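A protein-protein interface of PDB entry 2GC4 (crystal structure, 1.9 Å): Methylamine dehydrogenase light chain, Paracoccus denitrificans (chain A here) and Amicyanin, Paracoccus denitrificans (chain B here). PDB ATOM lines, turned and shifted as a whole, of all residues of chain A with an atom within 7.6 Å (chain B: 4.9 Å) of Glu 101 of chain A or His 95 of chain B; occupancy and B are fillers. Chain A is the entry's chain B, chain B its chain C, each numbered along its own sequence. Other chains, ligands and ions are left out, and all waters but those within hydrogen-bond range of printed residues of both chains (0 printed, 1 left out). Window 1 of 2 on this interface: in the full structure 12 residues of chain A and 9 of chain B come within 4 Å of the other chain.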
ATOM      1  N   ALA A  55      24.009  16.928   2.536  1.00  0.00           N
ATOM      2  CA  ALA A  55      24.493  17.046   3.908  1.00  0.00           C
ATOM      3  C   ALA A  55      25.766  16.227   4.102  1.00  0.00           C
ATOM      4  O   ALA A  55      26.078  15.357   3.290  1.00  0.00           O
ATOM      5  CB  ALA A  55      23.420  16.579   4.880  1.00  0.00           C
ATOM      6  N   SER A  56      26.501  16.510   5.172  1.00  0.00           N
ATOM      7  CA  SER A  56      27.728  15.775   5.451  1.00  0.00           C
ATOM      8  C   SER A  56      28.401  16.207   6.738  1.00  0.00           C
ATOM      9  O   SER A  56      28.035  17.215   7.347  1.00  0.00           O
ATOM     10  CB  SER A  56      28.733  15.970   4.318  1.00  0.00           C
ATOM     11  OG  SER A  56      29.284  17.275   4.365  1.00  0.00           O
ATOM     12  N   TRQ A  57      29.390  15.423   7.145  1.00  0.00           N
ATOM     13  CA  TRQ A  57      30.174  15.739   8.322  1.00  0.00           C
ATOM     14  C   TRQ A  57      31.375  16.466   7.719  1.00  0.00           C
ATOM     15  O   TRQ A  57      31.644  16.325   6.526  1.00  0.00           O
ATOM     16  CB  TRQ A  57      30.577  14.446   9.057  1.00  0.00           C
ATOM     17  CG  TRQ A  57      31.496  13.519   8.296  1.00  0.00           C
ATOM     18  CD1 TRQ A  57      32.862  13.586   8.282  1.00  0.00           C
ATOM     19  NE1 TRQ A  57      33.380  12.603   7.488  1.00  0.00           N
ATOM     20  CE2 TRQ A  57      32.353  11.868   6.962  1.00  0.00           C
ATOM     21  CZ2 TRQ A  57      32.414  10.773   6.093  1.00  0.00           C
ATOM     22  CH2 TRQ A  57      31.232  10.203   5.699  1.00  0.00           C
ATOM     23  CZ3 TRQ A  57      29.996  10.692   6.150  1.00  0.00           C
ATOM     24  CE3 TRQ A  57      29.923  11.780   7.017  1.00  0.00           C
ATOM     25  CD2 TRQ A  57      31.127  12.400   7.448  1.00  0.00           C
ATOM     26  O6  TRQ A  57      31.310   9.264   4.895  1.00  0.00           O
ATOM     27  O7  TRQ A  57      33.549  10.413   5.767  1.00  0.00           O
ATOM     28  N   VAL A  58      32.077  17.267   8.511  1.00  0.00           N
ATOM     29  CA  VAL A  58      33.226  17.994   7.981  1.00  0.00           C
ATOM     30  C   VAL A  58      34.453  17.802   8.851  1.00  0.00           C
ATOM     31  O   VAL A  58      34.383  17.223   9.935  1.00  0.00           O
ATOM     32  CB  VAL A  58      32.939  19.519   7.885  1.00  0.00           C
ATOM     33  CG1 VAL A  58      31.723  19.770   7.009  1.00  0.00           C
ATOM     34  CG2 VAL A  58      32.719  20.098   9.278  1.00  0.00           C
ATOM     35  N   ALA A  59      35.582  18.292   8.360  1.00  0.00           N
ATOM     36  CA  ALA A  59      36.830  18.218   9.097  1.00  0.00           C
ATOM     37  C   ALA A  59      37.790  19.252   8.549  1.00  0.00           C
ATOM     38  O   ALA A  59      37.743  19.593   7.370  1.00  0.00           O
ATOM     39  CB  ALA A  59      37.444  16.831   8.975  1.00  0.00           C
ATOM     40  N   ILE A  72      36.894  20.380   4.754  1.00  0.00           N
ATOM     41  CA  ILE A  72      36.475  19.388   3.766  1.00  0.00           C
ATOM     42  C   ILE A  72      35.070  18.901   4.110  1.00  0.00           C
ATOM     43  O   ILE A  72      34.803  18.553   5.261  1.00  0.00           O
ATOM     44  CB  ILE A  72      37.429  18.171   3.771  1.00  0.00           C
ATOM     45  CG1 ILE A  72      38.880  18.630   3.570  1.00  0.00           C
ATOM     46  CG2 ILE A  72      37.012  17.175   2.698  1.00  0.00           C
ATOM     47  CD1 ILE A  72      39.150  19.343   2.247  1.00  0.00           C
ATOM     48  N   GLY A  93      40.418  14.996  14.208  1.00  0.00           N
ATOM     49  CA  GLY A  93      39.426  15.911  14.744  1.00  0.00           C
ATOM     50  C   GLY A  93      38.018  15.341  14.803  1.00  0.00           C
ATOM     51  O   GLY A  93      37.060  16.067  15.080  1.00  0.00           O
ATOM     52  N   LEU A  95      34.804  13.776  16.197  1.00  0.00           N
ATOM     53  CA  LEU A  95      34.168  13.750  17.514  1.00  0.00           C
ATOM     54  C   LEU A  95      33.027  12.725  17.597  1.00  0.00           C
ATOM     55  O   LEU A  95      32.545  12.234  16.576  1.00  0.00           O
ATOM     56  CB  LEU A  95      33.640  15.151  17.851  1.00  0.00           C
ATOM     57  CG  LEU A  95      34.671  16.285  17.758  1.00  0.00           C
ATOM     58  CD1 LEU A  95      34.041  17.592  18.224  1.00  0.00           C
ATOM     59  CD2 LEU A  95      35.883  15.955  18.609  1.00  0.00           C
ATOM     60  N   PRO A  96      32.590  12.382  18.823  1.00  0.00           N
ATOM     61  CA  PRO A  96      31.509  11.414  19.042  1.00  0.00           C
ATOM     62  C   PRO A  96      30.201  11.823  18.367  1.00  0.00           C
ATOM     63  O   PRO A  96      30.034  12.973  17.958  1.00  0.00           O
ATOM     64  CB  PRO A  96      31.396  11.355  20.566  1.00  0.00           C
ATOM     65  CG  PRO A  96      32.802  11.634  21.013  1.00  0.00           C
ATOM     66  CD  PRO A  96      33.191  12.786  20.108  1.00  0.00           C
ATOM     67  N   VAL A  97      29.271  10.874  18.277  1.00  0.00           N
ATOM     68  CA  VAL A  97      27.992  11.098  17.613  1.00  0.00           C
ATOM     69  C   VAL A  97      27.142  12.252  18.153  1.00  0.00           C
ATOM     70  O   VAL A  97      26.299  12.787  17.425  1.00  0.00           O
ATOM     71  CB  VAL A  97      27.135   9.793  17.604  1.00  0.00           C
ATOM     72  CG1 VAL A  97      26.530   9.542  18.989  1.00  0.00           C
ATOM     73  CG2 VAL A  97      26.046   9.890  16.543  1.00  0.00           C
ATOM     74  N   TYR A  98      27.349  12.650  19.406  1.00  0.00           N
ATOM     75  CA  TYR A  98      26.563  13.750  19.959  1.00  0.00           C
ATOM     76  C   TYR A  98      27.079  15.116  19.484  1.00  0.00           C
ATOM     77  O   TYR A  98      26.588  16.164  19.902  1.00  0.00           O
ATOM     78  CB  TYR A  98      26.503  13.665  21.494  1.00  0.00           C
ATOM     79  CG  TYR A  98      27.832  13.762  22.206  1.00  0.00           C
ATOM     80  CD1 TYR A  98      28.339  14.999  22.616  1.00  0.00           C
ATOM     81  CD2 TYR A  98      28.575  12.615  22.494  1.00  0.00           C
ATOM     82  CE1 TYR A  98      29.554  15.086  23.304  1.00  0.00           C
ATOM     83  CE2 TYR A  98      29.785  12.692  23.176  1.00  0.00           C
ATOM     84  CZ  TYR A  98      30.268  13.931  23.580  1.00  0.00           C
ATOM     85  OH  TYR A  98      31.460  14.008  24.263  1.00  0.00           O
ATOM     86  N   ARG A  99      28.076  15.077  18.603  1.00  0.00           N
ATOM     87  CA  ARG A  99      28.652  16.267  17.972  1.00  0.00           C
ATOM     88  C   ARG A  99      28.690  15.810  16.514  1.00  0.00           C
ATOM     89  O   ARG A  99      29.753  15.715  15.901  1.00  0.00           O
ATOM     90  CB  ARG A  99      30.072  16.540  18.481  1.00  0.00           C
ATOM     91  CG  ARG A  99      30.155  17.043  19.924  1.00  0.00           C
ATOM     92  CD  ARG A  99      29.446  18.387  20.093  1.00  0.00           C
ATOM     93  NE  ARG A  99      30.041  19.431  19.261  1.00  0.00           N
ATOM     94  CZ  ARG A  99      31.211  20.013  19.507  1.00  0.00           C
ATOM     95  NH1 ARG A  99      31.667  20.949  18.684  1.00  0.00           N
ATOM     96  NH2 ARG A  99      31.919  19.676  20.580  1.00  0.00           N
ATOM     97  N   PRO A 100      27.507  15.525  15.943  1.00  0.00           N
ATOM     98  CA  PRO A 100      27.344  15.050  14.568  1.00  0.00           C
ATOM     99  C   PRO A 100      28.025  15.845  13.474  1.00  0.00           C
ATOM    100  O   PRO A 100      28.434  15.278  12.465  1.00  0.00           O
ATOM    101  CB  PRO A 100      25.827  14.987  14.398  1.00  0.00           C
ATOM    102  CG  PRO A 100      25.352  16.090  15.272  1.00  0.00           C
ATOM    103  CD  PRO A 100      26.205  15.930  16.508  1.00  0.00           C
ATOM    104  N   GLU A 101      28.156  17.154  13.668  1.00  0.00           N
ATOM    105  CA  GLU A 101      28.797  17.986  12.663  1.00  0.00           C
ATOM    106  C   GLU A 101      30.207  17.483  12.335  1.00  0.00           C
ATOM    107  O   GLU A 101      30.704  17.709  11.234  1.00  0.00           O
ATOM    108  CB  GLU A 101      28.846  19.453  13.124  1.00  0.00           C
ATOM    109  CG  GLU A 101      29.656  19.696  14.395  1.00  0.00           C
ATOM    110  CD  GLU A 101      28.802  19.715  15.654  1.00  0.00           C
ATOM    111  OE1 GLU A 101      27.842  18.919  15.747  1.00  0.00           O
ATOM    112  OE2 GLU A 101      29.100  20.523  16.561  1.00  0.00           O
ATOM    113  N   PHE A 102      30.850  16.793  13.279  1.00  0.00           N
ATOM    114  CA  PHE A 102      32.201  16.262  13.056  1.00  0.00           C
ATOM    115  C   PHE A 102      32.297  14.736  13.189  1.00  0.00           C
ATOM    116  O   PHE A 102      33.401  14.202  13.299  1.00  0.00           O
ATOM    117  CB  PHE A 102      33.199  16.869  14.052  1.00  0.00           C
ATOM    118  CG  PHE A 102      33.341  18.364  13.956  1.00  0.00           C
ATOM    119  CD1 PHE A 102      33.843  18.960  12.805  1.00  0.00           C
ATOM    120  CD2 PHE A 102      32.986  19.174  15.031  1.00  0.00           C
ATOM    121  CE1 PHE A 102      33.993  20.349  12.723  1.00  0.00           C
ATOM    122  CE2 PHE A 102      33.129  20.566  14.961  1.00  0.00           C
ATOM    123  CZ  PHE A 102      33.634  21.151  13.803  1.00  0.00           C
ATOM    124  N   ALA A 103      31.160  14.043  13.180  1.00  0.00           N
ATOM    125  CA  ALA A 103      31.139  12.580  13.355  1.00  0.00           C
ATOM    126  C   ALA A 103      31.130  11.825  12.029  1.00  0.00           C
ATOM    127  O   ALA A 103      30.288  12.108  11.173  1.00  0.00           O
ATOM    128  CB  ALA A 103      29.919  12.189  14.180  1.00  0.00           C
ATOM    129  N   ASN A 104      32.027  10.847  11.855  1.00  0.00           N
ATOM    130  CA  ASN A 104      32.048  10.142  10.577  1.00  0.00           C
ATOM    131  C   ASN A 104      31.576   8.685  10.476  1.00  0.00           C
ATOM    132  O   ASN A 104      31.849   8.026   9.477  1.00  0.00           O
ATOM    133  CB  ASN A 104      33.419  10.331   9.877  1.00  0.00           C
ATOM    134  CG  ASN A 104      34.556   9.498  10.483  1.00  0.00           C
ATOM    135  OD1 ASN A 104      35.724   9.684  10.118  1.00  0.00           O
ATOM    136  ND2 ASN A 104      34.229   8.577  11.377  1.00  0.00           N
ATOM    137  N   ILE A 106      28.373   8.141  10.781  1.00  0.00           N
ATOM    138  CA  ILE A 106      27.047   8.415  10.234  1.00  0.00           C
ATOM    139  C   ILE A 106      27.056   8.341   8.714  1.00  0.00           C
ATOM    140  O   ILE A 106      27.999   8.806   8.074  1.00  0.00           O
ATOM    141  CB  ILE A 106      26.566   9.829  10.648  1.00  0.00           C
ATOM    142  CG1 ILE A 106      26.426   9.905  12.168  1.00  0.00           C
ATOM    143  CG2 ILE A 106      25.235  10.168   9.963  1.00  0.00           C
ATOM    144  CD1 ILE A 106      26.090  11.286  12.688  1.00  0.00           C
ATOM    145  N   TRP A 108      26.271   9.858   5.703  1.00  0.00           N
ATOM    146  CA  TRP A 108      25.900  11.199   5.263  1.00  0.00           C
ATOM    147  C   TRP A 108      25.298  11.215   3.855  1.00  0.00           C
ATOM    148  O   TRP A 108      25.891  11.746   2.916  1.00  0.00           O
ATOM    149  CB  TRP A 108      27.126  12.127   5.372  1.00  0.00           C
ATOM    150  CG  TRP A 108      27.478  12.472   6.824  1.00  0.00           C
ATOM    151  CD1 TRP A 108      28.664  12.211   7.505  1.00  0.00           C
ATOM    152  CD2 TRP A 108      26.603  13.091   7.777  1.00  0.00           C
ATOM    153  NE1 TRP A 108      28.546  12.623   8.809  1.00  0.00           N
ATOM    154  CE2 TRP A 108      27.303  13.169   9.004  1.00  0.00           C
ATOM    155  CE3 TRP A 108      25.293  13.590   7.711  1.00  0.00           C
ATOM    156  CZ2 TRP A 108      26.735  13.726  10.157  1.00  0.00           C
ATOM    157  CZ3 TRP A 108      24.730  14.145   8.857  1.00  0.00           C
ATOM    158  CH2 TRP A 108      25.453  14.206  10.065  1.00  0.00           C
ATOM    159  N   MET B  28      27.318  28.090  14.350  1.00  0.00           N
ATOM    160  CA  MET B  28      26.334  27.025  14.527  1.00  0.00           C
ATOM    161  C   MET B  28      24.962  27.491  14.985  1.00  0.00           C
ATOM    162  O   MET B  28      24.296  26.795  15.753  1.00  0.00           O
ATOM    163  CB  MET B  28      26.858  25.985  15.525  1.00  0.00           C
ATOM    164  CG  MET B  28      28.189  25.370  15.149  1.00  0.00           C
ATOM    165  SD  MET B  28      28.124  24.524  13.566  1.00  0.00           S
ATOM    166  CE  MET B  28      27.390  22.976  14.044  1.00  0.00           C
ATOM    167  N   MET B  51      31.539  26.336   7.704  1.00  0.00           N
ATOM    168  CA  MET B  51      30.649  25.209   7.963  1.00  0.00           C
ATOM    169  C   MET B  51      29.360  25.356   7.147  1.00  0.00           C
ATOM    170  O   MET B  51      28.622  26.327   7.309  1.00  0.00           O
ATOM    171  CB  MET B  51      30.307  25.161   9.454  1.00  0.00           C
ATOM    172  CG  MET B  51      29.271  24.123   9.828  1.00  0.00           C
ATOM    173  SD  MET B  51      29.955  22.466   9.860  1.00  0.00           S
ATOM    174  CE  MET B  51      30.663  22.435  11.500  1.00  0.00           C
ATOM    175  N   PRO B  52      29.077  24.397   6.250  1.00  0.00           N
ATOM    176  CA  PRO B  52      27.859  24.467   5.433  1.00  0.00           C
ATOM    177  C   PRO B  52      26.584  24.305   6.264  1.00  0.00           C
ATOM    178  O   PRO B  52      26.561  23.535   7.224  1.00  0.00           O
ATOM    179  CB  PRO B  52      28.050  23.326   4.435  1.00  0.00           C
ATOM    180  CG  PRO B  52      29.558  23.249   4.296  1.00  0.00           C
ATOM    181  CD  PRO B  52      29.994  23.365   5.735  1.00  0.00           C
ATOM    182  N   HIS B  53      25.533  25.033   5.885  1.00  0.00           N
ATOM    183  CA  HIS B  53      24.237  24.993   6.576  1.00  0.00           C
ATOM    184  C   HIS B  53      23.105  25.166   5.558  1.00  0.00           C
ATOM    185  O   HIS B  53      23.332  25.608   4.437  1.00  0.00           O
ATOM    186  CB  HIS B  53      24.104  26.141   7.589  1.00  0.00           C
ATOM    187  CG  HIS B  53      25.147  26.153   8.663  1.00  0.00           C
ATOM    188  ND1 HIS B  53      25.212  25.239   9.690  1.00  0.00           N
ATOM    189  CD2 HIS B  53      26.143  27.042   8.901  1.00  0.00           C
ATOM    190  CE1 HIS B  53      26.212  25.598  10.506  1.00  0.00           C
ATOM    191  NE2 HIS B  53      26.812  26.689  10.070  1.00  0.00           N
ATOM    192  N   CYS B  92      18.446  22.752  10.687  1.00  0.00           N
ATOM    193  CA  CYS B  92      19.518  22.482   9.742  1.00  0.00           C
ATOM    194  C   CYS B  92      19.631  20.957   9.604  1.00  0.00           C
ATOM    195  O   CYS B  92      19.865  20.250  10.587  1.00  0.00           O
ATOM    196  CB  CYS B  92      20.818  23.070  10.272  1.00  0.00           C
ATOM    197  SG  CYS B  92      22.158  22.982   9.105  1.00  0.00           S
ATOM    198  N   THR B  93      19.461  20.460   8.383  1.00  0.00           N
ATOM    199  CA  THR B  93      19.493  19.025   8.116  1.00  0.00           C
ATOM    200  C   THR B  93      20.570  18.221   8.852  1.00  0.00           C
ATOM    201  O   THR B  93      20.241  17.347   9.645  1.00  0.00           O
ATOM    202  CB  THR B  93      19.581  18.762   6.597  1.00  0.00           C
ATOM    203  OG1 THR B  93      18.425  19.325   5.961  1.00  0.00           O
ATOM    204  CG2 THR B  93      19.628  17.260   6.310  1.00  0.00           C
ATOM    205  N   PRO B  94      21.863  18.505   8.613  1.00  0.00           N
ATOM    206  CA  PRO B  94      22.917  17.748   9.305  1.00  0.00           C
ATOM    207  C   PRO B  94      23.114  18.118  10.777  1.00  0.00           C
ATOM    208  O   PRO B  94      23.799  17.407  11.519  1.00  0.00           O
ATOM    209  CB  PRO B  94      24.162  18.056   8.472  1.00  0.00           C
ATOM    210  CG  PRO B  94      23.910  19.467   8.035  1.00  0.00           C
ATOM    211  CD  PRO B  94      22.449  19.437   7.629  1.00  0.00           C
ATOM    212  N   HIS B  95      22.508  19.226  11.195  1.00  0.00           N
ATOM    213  CA  HIS B  95      22.645  19.713  12.566  1.00  0.00           C
ATOM    214  C   HIS B  95      21.268  19.949  13.193  1.00  0.00           C
ATOM    215  O   HIS B  95      20.859  21.092  13.399  1.00  0.00           O
ATOM    216  CB  HIS B  95      23.444  21.021  12.548  1.00  0.00           C
ATOM    217  CG  HIS B  95      24.677  20.962  11.697  1.00  0.00           C
ATOM    218  ND1 HIS B  95      25.184  22.032  10.992  1.00  0.00           N
ATOM    219  CD2 HIS B  95      25.517  19.927  11.439  1.00  0.00           C
ATOM    220  CE1 HIS B  95      26.282  21.622  10.340  1.00  0.00           C
ATOM    221  NE2 HIS B  95      26.528  20.349  10.581  1.00  0.00           N
ATOM    222  N   PRO B  96      20.542  18.865  13.523  1.00  0.00           N
ATOM    223  CA  PRO B  96      19.203  18.930  14.125  1.00  0.00           C
ATOM    224  C   PRO B  96      19.069  19.873  15.321  1.00  0.00           C
ATOM    225  O   PRO B  96      17.979  20.380  15.600  1.00  0.00           O
ATOM    226  CB  PRO B  96      18.924  17.473  14.503  1.00  0.00           C
ATOM    227  CG  PRO B  96      19.668  16.709  13.453  1.00  0.00           C
ATOM    228  CD  PRO B  96      20.982  17.464  13.384  1.00  0.00           C
ATOM    229  N   PHE B  97      20.170  20.108  16.025  1.00  0.00           N
ATOM    230  CA  PHE B  97      20.152  20.993  17.184  1.00  0.00           C
ATOM    231  C   PHE B  97      20.030  22.468  16.797  1.00  0.00           C
ATOM    232  O   PHE B  97      19.735  23.316  17.646  1.00  0.00           O
ATOM    233  CB  PHE B  97      21.414  20.795  18.027  1.00  0.00           C
ATOM    234  CG  PHE B  97      22.684  20.882  17.240  1.00  0.00           C
ATOM    235  CD1 PHE B  97      23.131  19.794  16.495  1.00  0.00           C
ATOM    236  CD2 PHE B  97      23.429  22.056  17.225  1.00  0.00           C
ATOM    237  CE1 PHE B  97      24.302  19.878  15.744  1.00  0.00           C
ATOM    238  CE2 PHE B  97      24.602  22.151  16.477  1.00  0.00           C
ATOM    239  CZ  PHE B  97      25.038  21.059  15.736  1.00  0.00           C
ATOM    240  N   MET B  98      20.276  22.778  15.525  1.00  0.00           N
ATOM    241  CA  MET B  98      20.165  24.153  15.034  1.00  0.00           C
ATOM    242  C   MET B  98      18.719  24.393  14.652  1.00  0.00           C
ATOM    243  O   MET B  98      18.235  23.818  13.682  1.00  0.00           O
ATOM    244  CB  MET B  98      21.022  24.362  13.790  1.00  0.00           C
ATOM    245  CG  MET B  98      22.451  24.700  14.065  1.00  0.00           C
ATOM    246  SD  MET B  98      23.342  24.944  12.529  1.00  0.00           S
ATOM    247  CE  MET B  98      22.784  26.595  12.035  1.00  0.00           C
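Printed residues of chain B within 4 Å of Ala 55 of chain A: Pro 94 (3.95 Å). Gly 93 of chain A touches none of the printed residues of chain B. Glu 101 of chain A touches just these residues of chain B: Met 28 (3.9 Å), Met 51 (3.9 Å), His 95 (3.6 Å) and Phe 97 (3.5 Å). Of the printed residues of chain B, Phe 102 of chain A touches Met 51 (3.97 Å). Printed residues of chain A within 4 Å of Met 28 of chain B: Glu 101. His 95 of chain B touches just one residue of chain A: Glu 101 (3.6 Å). Pro 96 of chain B touches none of the printed residues of chain A. The nearest printed residue of chain B that does not touch Glu 101 of chain A is Pro 94 of chain B (4.9 Å).
CE3 of TRQ 57 of chain A is covalently linked to CD1 of Trp 108 of chain A. O of Glu 101 of chain A lies within hydrogen-bond range of N of Val 58 of chain A. O of Phe 102 of chain A lies within hydrogen-bond range of N of Leu 95 of chain A, 3.2 Å away. The guanidinium group of Arg 99 of chain A is in salt-bridge range of the side-chain carboxylate of Glu 101 of chain A. The backbone carbonyl oxygen (O) of Ala 103 of chain A is in hydrogen-bond range of NE1 of Trp 108 of chain A, 3.0 Å away. A ring nitrogen (NE2) of His 53 of chain B sits close to the backbone carbonyl oxygen (O) of Met 51 of chain B (3.3 Å).
Pro 94 of chain B touches Ala 55 of chain A (CB to CB, 3.95 Å). SD of Met 51 of chain B touches CG2 of Val 58 of chain A, 3.7 Å away. Phe 97 of chain B touches Pro 100 of chain A. CD of Glu 101 of chain A touches CE of Met 28 of chain B, 3.9 Å away. Glu 101 of chain A touches Met 51 of chain B (CB to CE, 3.9 Å). CB of Glu 101 of chain A touches NE2 of His 95 of chain B (3.6 Å). CZ of Phe 97 of chain B touches OE1 of Glu 101 of chain A, 3.5 Å away. CZ of Phe 102 of chain A touches CE of Met 51 of chain B, 3.97 Å away. Trp 108 of chain A touches Pro 94 of chain B.
Hydrophobic or aromatic side chains of chain A within 4 Å of the printed part of chain B: Ala 55, Val 58, Pro 100, Phe 102 and Trp 108. Of the 11 printed residues of chain B, 5 touch a printed residue of chain A. Hydrophobic or aromatic side chains of chain B within 4 Å of the printed part of chain A: Met 28, Met 51, Pro 94, His 95 and Phe 97. Among the printed residues, 9 pairs touch across the chains. Among the printed residues, no Asp or Glu carboxylate lies within 4 Å of a Lys or Arg side-chain nitrogen of the other chain.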
